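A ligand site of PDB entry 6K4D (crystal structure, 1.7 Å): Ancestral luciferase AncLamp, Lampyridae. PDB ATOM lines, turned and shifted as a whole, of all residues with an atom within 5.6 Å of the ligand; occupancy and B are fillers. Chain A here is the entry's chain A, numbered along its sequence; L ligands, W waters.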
ATOM      1  N   SER A 197       9.022  12.254  40.797  1.00  0.00           N
ATOM      2  CA  SER A 197       9.463  13.061  39.671  1.00  0.00           C
ATOM      3  C   SER A 197      10.829  13.659  39.982  1.00  0.00           C
ATOM      4  O   SER A 197      11.039  14.190  41.078  1.00  0.00           O
ATOM      5  CB  SER A 197       8.467  14.188  39.350  1.00  0.00           C
ATOM      6  OG  SER A 197       8.963  15.093  38.383  1.00  0.00           O
ATOM      7  N   ARG A 217      -8.896  17.951  38.128  1.00  0.00           N
ATOM      8  CA  ARG A 217      -8.828  16.932  37.076  1.00  0.00           C
ATOM      9  C   ARG A 217     -10.192  16.294  36.838  1.00  0.00           C
ATOM     10  O   ARG A 217     -10.582  16.049  35.687  1.00  0.00           O
ATOM     11  CB  ARG A 217      -7.799  15.855  37.447  1.00  0.00           C
ATOM     12  CG  ARG A 217      -7.885  14.604  36.531  1.00  0.00           C
ATOM     13  CD  ARG A 217      -7.488  14.936  35.089  1.00  0.00           C
ATOM     14  NE  ARG A 217      -7.781  13.821  34.191  1.00  0.00           N
ATOM     15  CZ  ARG A 217      -7.924  13.932  32.875  1.00  0.00           C
ATOM     16  NH1 ARG A 217      -7.778  15.115  32.302  1.00  0.00           N
ATOM     17  NH2 ARG A 217      -8.209  12.851  32.156  1.00  0.00           N
ATOM     18  N   HIS A 244       2.496   6.223  37.590  1.00  0.00           N
ATOM     19  CA  HIS A 244       2.911   7.522  37.077  1.00  0.00           C
ATOM     20  C   HIS A 244       1.689   8.431  36.951  1.00  0.00           C
ATOM     21  O   HIS A 244       0.578   7.967  36.750  1.00  0.00           O
ATOM     22  CB  HIS A 244       3.585   7.345  35.720  1.00  0.00           C
ATOM     23  CG  HIS A 244       4.249   8.581  35.201  1.00  0.00           C
ATOM     24  ND1 HIS A 244       3.547   9.622  34.621  1.00  0.00           N
ATOM     25  CD2 HIS A 244       5.548   8.954  35.187  1.00  0.00           C
ATOM     26  CE1 HIS A 244       4.396  10.564  34.257  1.00  0.00           C
ATOM     27  NE2 HIS A 244       5.610  10.189  34.597  1.00  0.00           N
ATOM     28  N   GLY A 245       1.916   9.741  37.109  1.00  0.00           N
ATOM     29  CA  GLY A 245       0.806  10.688  37.041  1.00  0.00           C
ATOM     30  C   GLY A 245      -0.003  10.567  35.759  1.00  0.00           C
ATOM     31  O   GLY A 245      -1.227  10.747  35.775  1.00  0.00           O
ATOM     32  N   PHE A 246       0.669  10.258  34.648  1.00  0.00           N
ATOM     33  CA  PHE A 246      -0.023  10.053  33.373  1.00  0.00           C
ATOM     34  C   PHE A 246      -1.085   8.965  33.503  1.00  0.00           C
ATOM     35  O   PHE A 246      -2.215   9.133  33.026  1.00  0.00           O
ATOM     36  CB  PHE A 246       1.017   9.709  32.304  1.00  0.00           C
ATOM     37  CG  PHE A 246       0.504   9.607  30.882  1.00  0.00           C
ATOM     38  CD1 PHE A 246      -0.785   9.984  30.533  1.00  0.00           C
ATOM     39  CD2 PHE A 246       1.342   9.112  29.883  1.00  0.00           C
ATOM     40  CE1 PHE A 246      -1.220   9.871  29.226  1.00  0.00           C
ATOM     41  CE2 PHE A 246       0.900   8.987  28.572  1.00  0.00           C
ATOM     42  CZ  PHE A 246      -0.377   9.377  28.240  1.00  0.00           C
ATOM     43  N   THR A 250      -5.469   9.958  34.731  1.00  0.00           N
ATOM     44  CA  THR A 250      -6.439   9.513  33.737  1.00  0.00           C
ATOM     45  C   THR A 250      -7.320   8.410  34.301  1.00  0.00           C
ATOM     46  O   THR A 250      -8.551   8.495  34.230  1.00  0.00           O
ATOM     47  CB  THR A 250      -5.745   9.033  32.458  1.00  0.00           C
ATOM     48  OG1 THR A 250      -4.729   8.076  32.790  1.00  0.00           O
ATOM     49  CG2 THR A 250      -5.144  10.211  31.695  1.00  0.00           C
ATOM     50  N   LEU A 285      -5.636   5.010  25.333  1.00  0.00           N
ATOM     51  CA  LEU A 285      -4.650   5.970  25.819  1.00  0.00           C
ATOM     52  C   LEU A 285      -3.276   5.383  25.569  1.00  0.00           C
ATOM     53  O   LEU A 285      -2.947   4.334  26.144  1.00  0.00           O
ATOM     54  CB  LEU A 285      -4.851   6.261  27.305  1.00  0.00           C
ATOM     55  CG  LEU A 285      -3.936   7.307  27.911  1.00  0.00           C
ATOM     56  CD1 LEU A 285      -4.191   8.640  27.227  1.00  0.00           C
ATOM     57  CD2 LEU A 285      -4.143   7.402  29.420  1.00  0.00           C
ATOM     58  N   ALA A 312      -5.854   8.523  21.851  1.00  0.00           N
ATOM     59  CA  ALA A 312      -5.171   9.587  22.583  1.00  0.00           C
ATOM     60  C   ALA A 312      -3.705   9.241  22.777  1.00  0.00           C
ATOM     61  O   ALA A 312      -3.359   8.071  23.004  1.00  0.00           O
ATOM     62  CB  ALA A 312      -5.828   9.809  23.951  1.00  0.00           C
ATOM     63  N   SER A 313      -2.839  10.261  22.705  1.00  0.00           N
ATOM     64  CA  SER A 313      -1.418  10.121  22.996  1.00  0.00           C
ATOM     65  C   SER A 313      -1.008  11.131  24.048  1.00  0.00           C
ATOM     66  O   SER A 313      -1.626  12.197  24.170  1.00  0.00           O
ATOM     67  CB  SER A 313      -0.579  10.303  21.701  1.00  0.00           C
ATOM     68  OG  SER A 313       0.824  10.261  21.950  1.00  0.00           O
ATOM     69  N   GLY A 314      -0.004  10.781  24.837  1.00  0.00           N
ATOM     70  CA  GLY A 314       0.599  11.755  25.735  1.00  0.00           C
ATOM     71  C   GLY A 314       1.978  11.276  26.142  1.00  0.00           C
ATOM     72  O   GLY A 314       2.435  10.210  25.710  1.00  0.00           O
ATOM     73  N   GLY A 315       2.639  12.078  26.972  1.00  0.00           N
ATOM     74  CA  GLY A 315       3.887  11.672  27.603  1.00  0.00           C
ATOM     75  C   GLY A 315       5.155  12.105  26.895  1.00  0.00           C
ATOM     76  O   GLY A 315       6.204  12.207  27.546  1.00  0.00           O
ATOM     77  N   ALA A 316       5.095  12.380  25.604  1.00  0.00           N
ATOM     78  CA  ALA A 316       6.289  12.672  24.811  1.00  0.00           C
ATOM     79  C   ALA A 316       5.839  13.264  23.472  1.00  0.00           C
ATOM     80  O   ALA A 316       4.687  13.068  23.074  1.00  0.00           O
ATOM     81  CB  ALA A 316       7.127  11.411  24.564  1.00  0.00           C
ATOM     82  N   PRO A 317       6.733  13.978  22.782  1.00  0.00           N
ATOM     83  CA  PRO A 317       6.344  14.586  21.501  1.00  0.00           C
ATOM     84  C   PRO A 317       5.747  13.593  20.517  1.00  0.00           C
ATOM     85  O   PRO A 317       6.295  12.509  20.281  1.00  0.00           O
ATOM     86  CB  PRO A 317       7.668  15.167  20.977  1.00  0.00           C
ATOM     87  CG  PRO A 317       8.423  15.522  22.225  1.00  0.00           C
ATOM     88  CD  PRO A 317       8.072  14.426  23.221  1.00  0.00           C
ATOM     89  N   LEU A 318       4.609  13.963  19.937  1.00  0.00           N
ATOM     90  CA  LEU A 318       3.972  13.186  18.870  1.00  0.00           C
ATOM     91  C   LEU A 318       4.136  13.916  17.544  1.00  0.00           C
ATOM     92  O   LEU A 318       3.818  15.114  17.449  1.00  0.00           O
ATOM     93  CB  LEU A 318       2.491  12.987  19.172  1.00  0.00           C
ATOM     94  CG  LEU A 318       1.724  12.250  18.070  1.00  0.00           C
ATOM     95  CD1 LEU A 318       2.137  10.786  18.039  1.00  0.00           C
ATOM     96  CD2 LEU A 318       0.208  12.382  18.290  1.00  0.00           C
ATOM     97  N   ARG A 336      -6.708  12.572  19.717  1.00  0.00           N
ATOM     98  CA  ARG A 336      -6.725  13.255  21.007  1.00  0.00           C
ATOM     99  C   ARG A 336      -5.302  13.333  21.543  1.00  0.00           C
ATOM    100  O   ARG A 336      -4.515  12.390  21.368  1.00  0.00           O
ATOM    101  CB  ARG A 336      -7.640  12.528  21.999  1.00  0.00           C
ATOM    102  CG  ARG A 336      -7.699  13.120  23.394  1.00  0.00           C
ATOM    103  CD  ARG A 336      -8.788  12.422  24.224  1.00  0.00           C
ATOM    104  NE  ARG A 336      -8.937  13.053  25.544  1.00  0.00           N
ATOM    105  CZ  ARG A 336      -9.668  14.144  25.764  1.00  0.00           C
ATOM    106  NH1 ARG A 336     -10.341  14.716  24.767  1.00  0.00           N
ATOM    107  NH2 ARG A 336      -9.704  14.668  26.979  1.00  0.00           N
ATOM    108  N   GLN A 337      -4.972  14.425  22.227  1.00  0.00           N
ATOM    109  CA  GLN A 337      -3.651  14.520  22.812  1.00  0.00           C
ATOM    110  C   GLN A 337      -3.710  15.388  24.068  1.00  0.00           C
ATOM    111  O   GLN A 337      -4.553  16.277  24.195  1.00  0.00           O
ATOM    112  CB  GLN A 337      -2.608  15.082  21.822  1.00  0.00           C
ATOM    113  CG  GLN A 337      -1.171  14.875  22.328  1.00  0.00           C
ATOM    114  CD  GLN A 337      -0.077  15.358  21.395  1.00  0.00           C
ATOM    115  OE1 GLN A 337       1.105  15.315  21.752  1.00  0.00           O
ATOM    116  NE2 GLN A 337      -0.454  15.794  20.189  1.00  0.00           N
ATOM    117  N   GLY A 338      -2.812  15.106  24.994  1.00  0.00           N
ATOM    118  CA  GLY A 338      -2.675  15.918  26.182  1.00  0.00           C
ATOM    119  C   GLY A 338      -1.211  16.077  26.515  1.00  0.00           C
ATOM    120  O   GLY A 338      -0.372  15.247  26.144  1.00  0.00           O
ATOM    121  N   TYR A 339      -0.922  17.149  27.257  1.00  0.00           N
ATOM    122  CA  TYR A 339       0.442  17.448  27.671  1.00  0.00           C
ATOM    123  C   TYR A 339       0.375  17.894  29.114  1.00  0.00           C
ATOM    124  O   TYR A 339      -0.480  18.710  29.477  1.00  0.00           O
ATOM    125  CB  TYR A 339       1.065  18.548  26.791  1.00  0.00           C
ATOM    126  CG  TYR A 339       2.214  19.291  27.440  1.00  0.00           C
ATOM    127  CD1 TYR A 339       3.536  18.948  27.169  1.00  0.00           C
ATOM    128  CD2 TYR A 339       1.982  20.362  28.292  1.00  0.00           C
ATOM    129  CE1 TYR A 339       4.589  19.647  27.755  1.00  0.00           C
ATOM    130  CE2 TYR A 339       3.018  21.057  28.893  1.00  0.00           C
ATOM    131  CZ  TYR A 339       4.316  20.698  28.612  1.00  0.00           C
ATOM    132  OH  TYR A 339       5.341  21.401  29.209  1.00  0.00           O
ATOM    133  N   GLY A 340       1.283  17.377  29.938  1.00  0.00           N
ATOM    134  CA  GLY A 340       1.364  17.838  31.310  1.00  0.00           C
ATOM    135  C   GLY A 340       2.623  17.301  31.934  1.00  0.00           C
ATOM    136  O   GLY A 340       3.428  16.646  31.275  1.00  0.00           O
ATOM    137  N   LEU A 341       2.779  17.574  33.234  1.00  0.00           N
ATOM    138  CA  LEU A 341       3.912  17.121  34.010  1.00  0.00           C
ATOM    139  C   LEU A 341       3.411  16.536  35.315  1.00  0.00           C
ATOM    140  O   LEU A 341       2.319  16.874  35.782  1.00  0.00           O
ATOM    141  CB  LEU A 341       4.910  18.257  34.333  1.00  0.00           C
ATOM    142  CG  LEU A 341       5.618  19.057  33.234  1.00  0.00           C
ATOM    143  CD1 LEU A 341       4.703  20.119  32.595  1.00  0.00           C
ATOM    144  CD2 LEU A 341       6.870  19.712  33.819  1.00  0.00           C
ATOM    145  N   THR A 342       4.214  15.664  35.927  1.00  0.00           N
ATOM    146  CA  THR A 342       3.852  15.185  37.263  1.00  0.00           C
ATOM    147  C   THR A 342       3.497  16.350  38.172  1.00  0.00           C
ATOM    148  O   THR A 342       2.515  16.284  38.937  1.00  0.00           O
ATOM    149  CB  THR A 342       5.006  14.365  37.854  1.00  0.00           C
ATOM    150  OG1 THR A 342       5.269  13.240  37.009  1.00  0.00           O
ATOM    151  CG2 THR A 342       4.659  13.870  39.269  1.00  0.00           C
ATOM    152  N   GLU A 343       4.231  17.461  38.046  1.00  0.00           N
ATOM    153  CA  GLU A 343       4.066  18.620  38.900  1.00  0.00           C
ATOM    154  C   GLU A 343       2.794  19.403  38.593  1.00  0.00           C
ATOM    155  O   GLU A 343       2.435  20.289  39.380  1.00  0.00           O
ATOM    156  CB  GLU A 343       5.278  19.537  38.749  1.00  0.00           C
ATOM    157  CG  GLU A 343       6.563  19.028  39.428  1.00  0.00           C
ATOM    158  CD  GLU A 343       7.382  18.077  38.556  1.00  0.00           C
ATOM    159  OE1 GLU A 343       6.906  17.647  37.484  1.00  0.00           O
ATOM    160  OE2 GLU A 343       8.521  17.757  38.968  1.00  0.00           O
ATOM    161  N   THR A 345      -0.161  17.744  38.060  1.00  0.00           N
ATOM    162  CA  THR A 345      -1.144  16.687  38.276  1.00  0.00           C
ATOM    163  C   THR A 345      -1.416  15.903  36.995  1.00  0.00           C
ATOM    164  O   THR A 345      -1.118  14.709  36.922  1.00  0.00           O
ATOM    165  CB  THR A 345      -2.461  17.218  38.856  1.00  0.00           C
ATOM    166  OG1 THR A 345      -2.197  17.947  40.053  1.00  0.00           O
ATOM    167  CG2 THR A 345      -3.409  16.047  39.216  1.00  0.00           C
ATOM    168  N   SER A 346      -2.005  16.547  35.994  1.00  0.00           N
ATOM    169  CA  SER A 346      -2.435  15.870  34.791  1.00  0.00           C
ATOM    170  C   SER A 346      -2.191  16.805  33.610  1.00  0.00           C
ATOM    171  O   SER A 346      -1.420  17.762  33.701  1.00  0.00           O
ATOM    172  CB  SER A 346      -3.905  15.425  34.915  1.00  0.00           C
ATOM    173  OG  SER A 346      -4.263  14.550  33.872  1.00  0.00           O
ATOM    174  N   ALA A 347      -2.883  16.549  32.503  1.00  0.00           N
ATOM    175  CA  ALA A 347      -2.690  17.358  31.303  1.00  0.00           C
ATOM    176  C   ALA A 347      -3.263  18.755  31.524  1.00  0.00           C
ATOM    177  O   ALA A 347      -4.397  18.918  31.981  1.00  0.00           O
ATOM    178  CB  ALA A 347      -3.366  16.705  30.092  1.00  0.00           C
ATOM    179  N   ILE A 350      -4.905  20.259  26.349  1.00  0.00           N
ATOM    180  CA  ILE A 350      -5.690  19.131  25.851  1.00  0.00           C
ATOM    181  C   ILE A 350      -6.347  19.561  24.547  1.00  0.00           C
ATOM    182  O   ILE A 350      -6.782  20.711  24.413  1.00  0.00           O
ATOM    183  CB  ILE A 350      -6.766  18.705  26.872  1.00  0.00           C
ATOM    184  CG1 ILE A 350      -6.119  18.149  28.139  1.00  0.00           C
ATOM    185  CG2 ILE A 350      -7.680  17.618  26.284  1.00  0.00           C
ATOM    186  CD1 ILE A 350      -7.134  17.728  29.195  1.00  0.00           C
ATOM    187  N   THR A 361      -0.760  19.847  20.614  1.00  0.00           N
ATOM    188  CA  THR A 361      -1.309  19.054  21.699  1.00  0.00           C
ATOM    189  C   THR A 361      -2.530  19.712  22.348  1.00  0.00           C
ATOM    190  O   THR A 361      -3.004  19.225  23.392  1.00  0.00           O
ATOM    191  CB  THR A 361      -0.206  18.771  22.747  1.00  0.00           C
ATOM    192  OG1 THR A 361      -0.711  17.823  23.707  1.00  0.00           O
ATOM    193  CG2 THR A 361       0.271  20.053  23.472  1.00  0.00           C
ATOM    194  N   SER A 419       8.348  24.565  32.980  1.00  0.00           N
ATOM    195  CA  SER A 419       8.221  23.164  32.606  1.00  0.00           C
ATOM    196  C   SER A 419       9.524  22.528  32.151  1.00  0.00           C
ATOM    197  O   SER A 419       9.645  21.292  32.210  1.00  0.00           O
ATOM    198  CB  SER A 419       7.207  23.006  31.468  1.00  0.00           C
ATOM    199  OG  SER A 419       7.705  23.590  30.280  1.00  0.00           O
ATOM    200  N   ASP A 421      10.318  22.615  29.067  1.00  0.00           N
ATOM    201  CA  ASP A 421       9.988  22.270  27.694  1.00  0.00           C
ATOM    202  C   ASP A 421       9.989  23.529  26.834  1.00  0.00           C
ATOM    203  O   ASP A 421       9.594  24.600  27.301  1.00  0.00           O
ATOM    204  CB  ASP A 421       8.611  21.609  27.610  1.00  0.00           C
ATOM    205  CG  ASP A 421       8.555  20.316  28.380  1.00  0.00           C
ATOM    206  OD1 ASP A 421       9.460  19.472  28.184  1.00  0.00           O
ATOM    207  OD2 ASP A 421       7.602  20.144  29.191  1.00  0.00           O
ATOM    208  N   ILE A 433       4.522  21.448  21.150  1.00  0.00           N
ATOM    209  CA  ILE A 433       5.689  21.117  21.961  1.00  0.00           C
ATOM    210  C   ILE A 433       6.845  20.781  21.035  1.00  0.00           C
ATOM    211  O   ILE A 433       6.725  19.903  20.170  1.00  0.00           O
ATOM    212  CB  ILE A 433       5.390  19.940  22.905  1.00  0.00           C
ATOM    213  CG1 ILE A 433       4.022  20.100  23.584  1.00  0.00           C
ATOM    214  CG2 ILE A 433       6.541  19.782  23.950  1.00  0.00           C
ATOM    215  CD1 ILE A 433       3.840  21.378  24.409  1.00  0.00           C
ATOM    216  N   ASP A 435      10.371  20.165  22.175  1.00  0.00           N
ATOM    217  CA  ASP A 435      11.176  19.159  22.862  1.00  0.00           C
ATOM    218  C   ASP A 435      11.438  19.633  24.273  1.00  0.00           C
ATOM    219  O   ASP A 435      11.245  20.822  24.581  1.00  0.00           O
ATOM    220  CB  ASP A 435      12.527  18.923  22.160  1.00  0.00           C
ATOM    221  CG  ASP A 435      12.615  17.572  21.475  1.00  0.00           C
ATOM    222  OD1 ASP A 435      12.103  16.568  21.997  1.00  0.00           O
ATOM    223  OD2 ASP A 435      13.218  17.504  20.390  1.00  0.00           O
ATOM    224  N   ARG A 436      11.914  18.735  25.133  1.00  0.00           N
ATOM    225  CA  ARG A 436      12.504  19.132  26.407  1.00  0.00           C
ATOM    226  C   ARG A 436      13.800  19.904  26.136  1.00  0.00           C
ATOM    227  O   ARG A 436      14.588  19.511  25.278  1.00  0.00           O
ATOM    228  CB  ARG A 436      12.796  17.902  27.264  1.00  0.00           C
ATOM    229  CG  ARG A 436      13.013  18.241  28.701  1.00  0.00           C
ATOM    230  CD  ARG A 436      12.704  17.073  29.610  1.00  0.00           C
ATOM    231  NE  ARG A 436      12.804  17.446  31.015  1.00  0.00           N
ATOM    232  CZ  ARG A 436      11.942  18.240  31.653  1.00  0.00           C
ATOM    233  NH1 ARG A 436      10.889  18.775  31.012  1.00  0.00           N
ATOM    234  NH2 ARG A 436      12.116  18.507  32.938  1.00  0.00           N
ATOM    235  N   THR A 526       6.266   5.975  29.991  1.00  0.00           N
ATOM    236  CA  THR A 526       5.406   7.062  29.526  1.00  0.00           C
ATOM    237  C   THR A 526       5.913   7.699  28.228  1.00  0.00           C
ATOM    238  O   THR A 526       5.472   8.794  27.872  1.00  0.00           O
ATOM    239  CB  THR A 526       5.206   8.122  30.605  1.00  0.00           C
ATOM    240  OG1 THR A 526       6.447   8.751  30.935  1.00  0.00           O
ATOM    241  CG2 THR A 526       4.584   7.508  31.871  1.00  0.00           C
ATOM    242  N   LYS A 528       9.160   8.473  27.325  1.00  0.00           N
ATOM    243  CA  LYS A 528      10.360   9.285  27.375  1.00  0.00           C
ATOM    244  C   LYS A 528      11.513   8.529  26.735  1.00  0.00           C
ATOM    245  O   LYS A 528      11.826   7.414  27.147  1.00  0.00           O
ATOM    246  CB  LYS A 528      10.702   9.645  28.819  1.00  0.00           C
ATOM    247  CG  LYS A 528       9.982  10.854  29.376  1.00  0.00           C
ATOM    248  CD  LYS A 528       8.525  10.567  29.562  1.00  0.00           C
ATOM    249  CE  LYS A 528       7.843  11.653  30.370  1.00  0.00           C
ATOM    250  NZ  LYS A 528       6.377  11.537  30.234  1.00  0.00           N
HETATM  251  C1  LIG L   1      -4.738  12.746  28.811  1.00  0.00           C
HETATM  252  C2  LIG L   1       7.344  15.740  30.465  1.00  0.00           C
HETATM  253  C3  LIG L   1       7.388  16.972  28.511  1.00  0.00           C
HETATM  254  C4  LIG L   1       2.276  13.879  33.926  1.00  0.00           C
HETATM  255  C5  LIG L   1       2.789  13.017  32.748  1.00  0.00           C
HETATM  256  C6  LIG L   1       0.819  13.710  31.819  1.00  0.00           C
HETATM  257  C7  LIG L   1      -0.574  13.504  31.069  1.00  0.00           C
HETATM  258  C8  LIG L   1      -2.689  13.155  30.112  1.00  0.00           C
HETATM  259  C9  LIG L   1      -1.982  13.079  28.884  1.00  0.00           C
HETATM  260  C10 LIG L   1      -2.615  12.806  27.615  1.00  0.00           C
HETATM  261  C11 LIG L   1      -4.008  12.687  27.572  1.00  0.00           C
HETATM  262  C12 LIG L   1      -4.109  12.967  30.041  1.00  0.00           C
HETATM  263  C13 LIG L   1       4.335  13.202  32.620  1.00  0.00           C
HETATM  264  C14 LIG L   1       6.738  15.440  31.883  1.00  0.00           C
HETATM  265  C15 LIG L   1       7.014  17.170  30.041  1.00  0.00           C
HETATM  266  C16 LIG L   1       6.914  15.488  28.222  1.00  0.00           C
HETATM  267  C17 LIG L   1       4.293  15.055  28.310  1.00  0.00           C
HETATM  268  C18 LIG L   1       3.754  15.570  26.231  1.00  0.00           C
HETATM  269  C19 LIG L   1       5.152  15.772  26.348  1.00  0.00           C
HETATM  270  C20 LIG L   1       5.292  16.439  24.169  1.00  0.00           C
HETATM  271  C21 LIG L   1       3.132  15.823  24.947  1.00  0.00           C
HETATM  272  N1  LIG L   1       2.074  13.567  31.486  1.00  0.00           N
HETATM  273  N2  LIG L   1      -1.870  13.339  31.360  1.00  0.00           N
HETATM  274  N3  LIG L   1       5.501  15.464  27.684  1.00  0.00           N
HETATM  275  N4  LIG L   1       3.259  15.089  27.461  1.00  0.00           N
HETATM  276  N5  LIG L   1       5.943  16.233  25.328  1.00  0.00           N
HETATM  277  N6  LIG L   1       3.942  16.288  23.934  1.00  0.00           N
HETATM  278  N7  LIG L   1       1.762  15.657  24.768  1.00  0.00           N
HETATM  279  O1  LIG L   1      -4.728  12.476  26.425  1.00  0.00           O
HETATM  280  O2  LIG L   1       4.757  12.987  31.496  1.00  0.00           O
HETATM  281  O3  LIG L   1       4.867  13.449  33.504  1.00  0.00           O
HETATM  282  O4  LIG L   1       7.206  12.140  33.759  1.00  0.00           O
HETATM  283  O5  LIG L   1       6.767  14.448  34.734  1.00  0.00           O
HETATM  284  O6  LIG L   1       7.129  14.157  32.149  1.00  0.00           O
HETATM  285  O7  LIG L   1       6.838  14.851  29.439  1.00  0.00           O
HETATM  286  O8  LIG L   1       8.746  16.998  28.340  1.00  0.00           O
HETATM  287  O9  LIG L   1       7.782  18.007  30.808  1.00  0.00           O
HETATM  288  P1  LIG L   1       6.641  13.464  33.676  1.00  0.00           P
HETATM  289  S1  LIG L   1       0.505  13.862  33.475  1.00  0.00           S
HETATM  290  S2  LIG L   1      -0.248  13.365  29.322  1.00  0.00           S
HETATM  291  O   HOH W   1       9.292  10.231  33.283  1.00  0.00           O
HETATM  292  O   HOH W   2       9.413  17.375  32.966  1.00  0.00           O
HETATM  293  O   HOH W   3      -2.730  12.338  33.953  1.00  0.00           O
HETATM  294  O   HOH W   4      10.211  14.576  28.796  1.00  0.00           O
HETATM  295  O   HOH W   5      10.494  14.860  31.813  1.00  0.00           O
HETATM  296  O   HOH W   6       8.074  12.246  36.858  1.00  0.00           O
HETATM  297  O   HOH W   7      -7.471  11.474  27.396  1.00  0.00           O
HETATM  298  O   HOH W   8       3.314  16.675  21.282  1.00  0.00           O
HETATM  299  O   HOH W   9       8.526  16.511  35.572  1.00  0.00           O
HETATM  300  O   HOH W  10       8.810  17.148  25.409  1.00  0.00           O
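The backbone carbonyl oxygen (O) of Ala 316 lies close to a nitrogen (N6) of the ligand (3.4 Å).
N of Pro 317 sits close to N5 of the ligand (3.5 Å).
O of Gly 340 sits close to N1 of the ligand.
Residues that only touch the ligand: Thr 250 (3.4 Å), Leu 285 (3.96 Å), Ala 312 (3.8 Å), Ser 313 (3.6 Å), Gly 314 (3.9 Å), Tyr 339 (3.5 Å), Leu 341 (3.2 Å), Thr 345 (3.9 Å), Ser 346 (3.7 Å), Ala 347 (3.6 Å) and Ile 433 (3.6 Å).
Within 4 Å of the ligand: His 244, Phe 246, Thr 250, Leu 285, Ala 312, Ser 313, Gly 314, Gly 315, Ala 316, Pro 317, Gln 337, Gly 338, Tyr 339, Gly 340, Leu 341, Thr 342, Thr 345, Ser 346, Ala 347, Thr 361, Asp 421, Ile 433, Arg 436 and Lys 528.
The nearest printed residue that does not touch the ligand is Ser 419 (4.03 Å).
Water W8 lies within hydrogen-bond range of OE1 of Gln 337 (2.6 Å), N6 of the ligand (2.8 Å) and N of Leu 318 (3.3 Å).
Water W2 bridges O9 of the ligand and NH1 of Arg 436.
Water W9 lies within hydrogen-bond range of the side-chain carboxylate (OE1) of Glu 343, an oxygen (O5) of the ligand and the side-chain hydroxyl (OG) of Ser 197.
Water W10 lies within hydrogen-bond range of an oxygen (O8) of the ligand and the backbone NH (N) of Arg 436.
Water W7 bridges the guanidinium group (NE) of Arg 336 (2.8 Å) and an oxygen (O1) of the ligand (3.1 Å).
Water W6 lies within hydrogen-bond range of the side-chain hydroxyl of Thr 342 (3.0 Å), an oxygen (O4) of the ligand (3.2 Å) and the side-chain hydroxyl of Ser 197 (3.3 Å).
ND1 of His 244 is in hydrogen-bond range of N of Phe 246 (2.9 Å).
OD2 of Asp 421 lies within hydrogen-bond range of OH of Tyr 339.
The backbone NH of Gly 338 is in hydrogen-bond range of the backbone carbonyl oxygen of Ser 313 (3.2 Å).
The backbone carbonyl oxygen (O) of Phe 246 sits at hydrogen-bond distance from the side-chain hydroxyl (OG1) of Thr 250, at 2.7 Å.
The backbone carbonyl oxygen of Arg 336 sits at hydrogen-bond distance from the backbone NH of Ser 313 (3.0 Å).
The side-chain carboxylate of Asp 421 lies within salt-bridge range of the guanidinium group of Arg 436, 3.2 Å away.
The side-chain hydroxyl (OG) of Ser 419 lies close to the side-chain hydroxyl (OH) of Tyr 339 (3.4 Å).
The side-chain hydroxyl (OG1) of Thr 526 lies within hydrogen-bond range of the side-chain amino group (NZ) of Lys 528, at 2.9 Å.
The side-chain amino group (NZ) of Lys 528 is in salt-bridge range of an oxygen (O4) of the ligand (3.7 Å).
A ring nitrogen (NE2) of His 244 is in hydrogen-bond range of an oxygen (O4) of the ligand, 2.7 Å away.
A nitrogen (N7) of the ligand sits at hydrogen-bond distance from the side-chain amide oxygen (OE1) of Gln 337.
The side-chain hydroxyl of Thr 342 lies within hydrogen-bond range of an oxygen (O5) of the ligand (3.0 Å).
N of Phe 246 sits close to S1 of the ligand (3.8 Å).
The side-chain carboxylate (OD1) of Asp 421 sits at hydrogen-bond distance from an oxygen (O8) of the ligand (2.6 Å).
NH1 of Arg 436 sits at hydrogen-bond distance from O9 of the ligand (3.2 Å).
N4 of the ligand sits at hydrogen-bond distance from N of Gly 315 (3.1 Å).
The side-chain hydroxyl of Thr 361 is in hydrogen-bond range of a nitrogen (N7) of the ligand (3.5 Å).
The backbone NH of Thr 342 is in hydrogen-bond range of an oxygen (O5) of the ligand (3.1 Å).
N7 of the ligand sits at hydrogen-bond distance from O of Gly 338.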
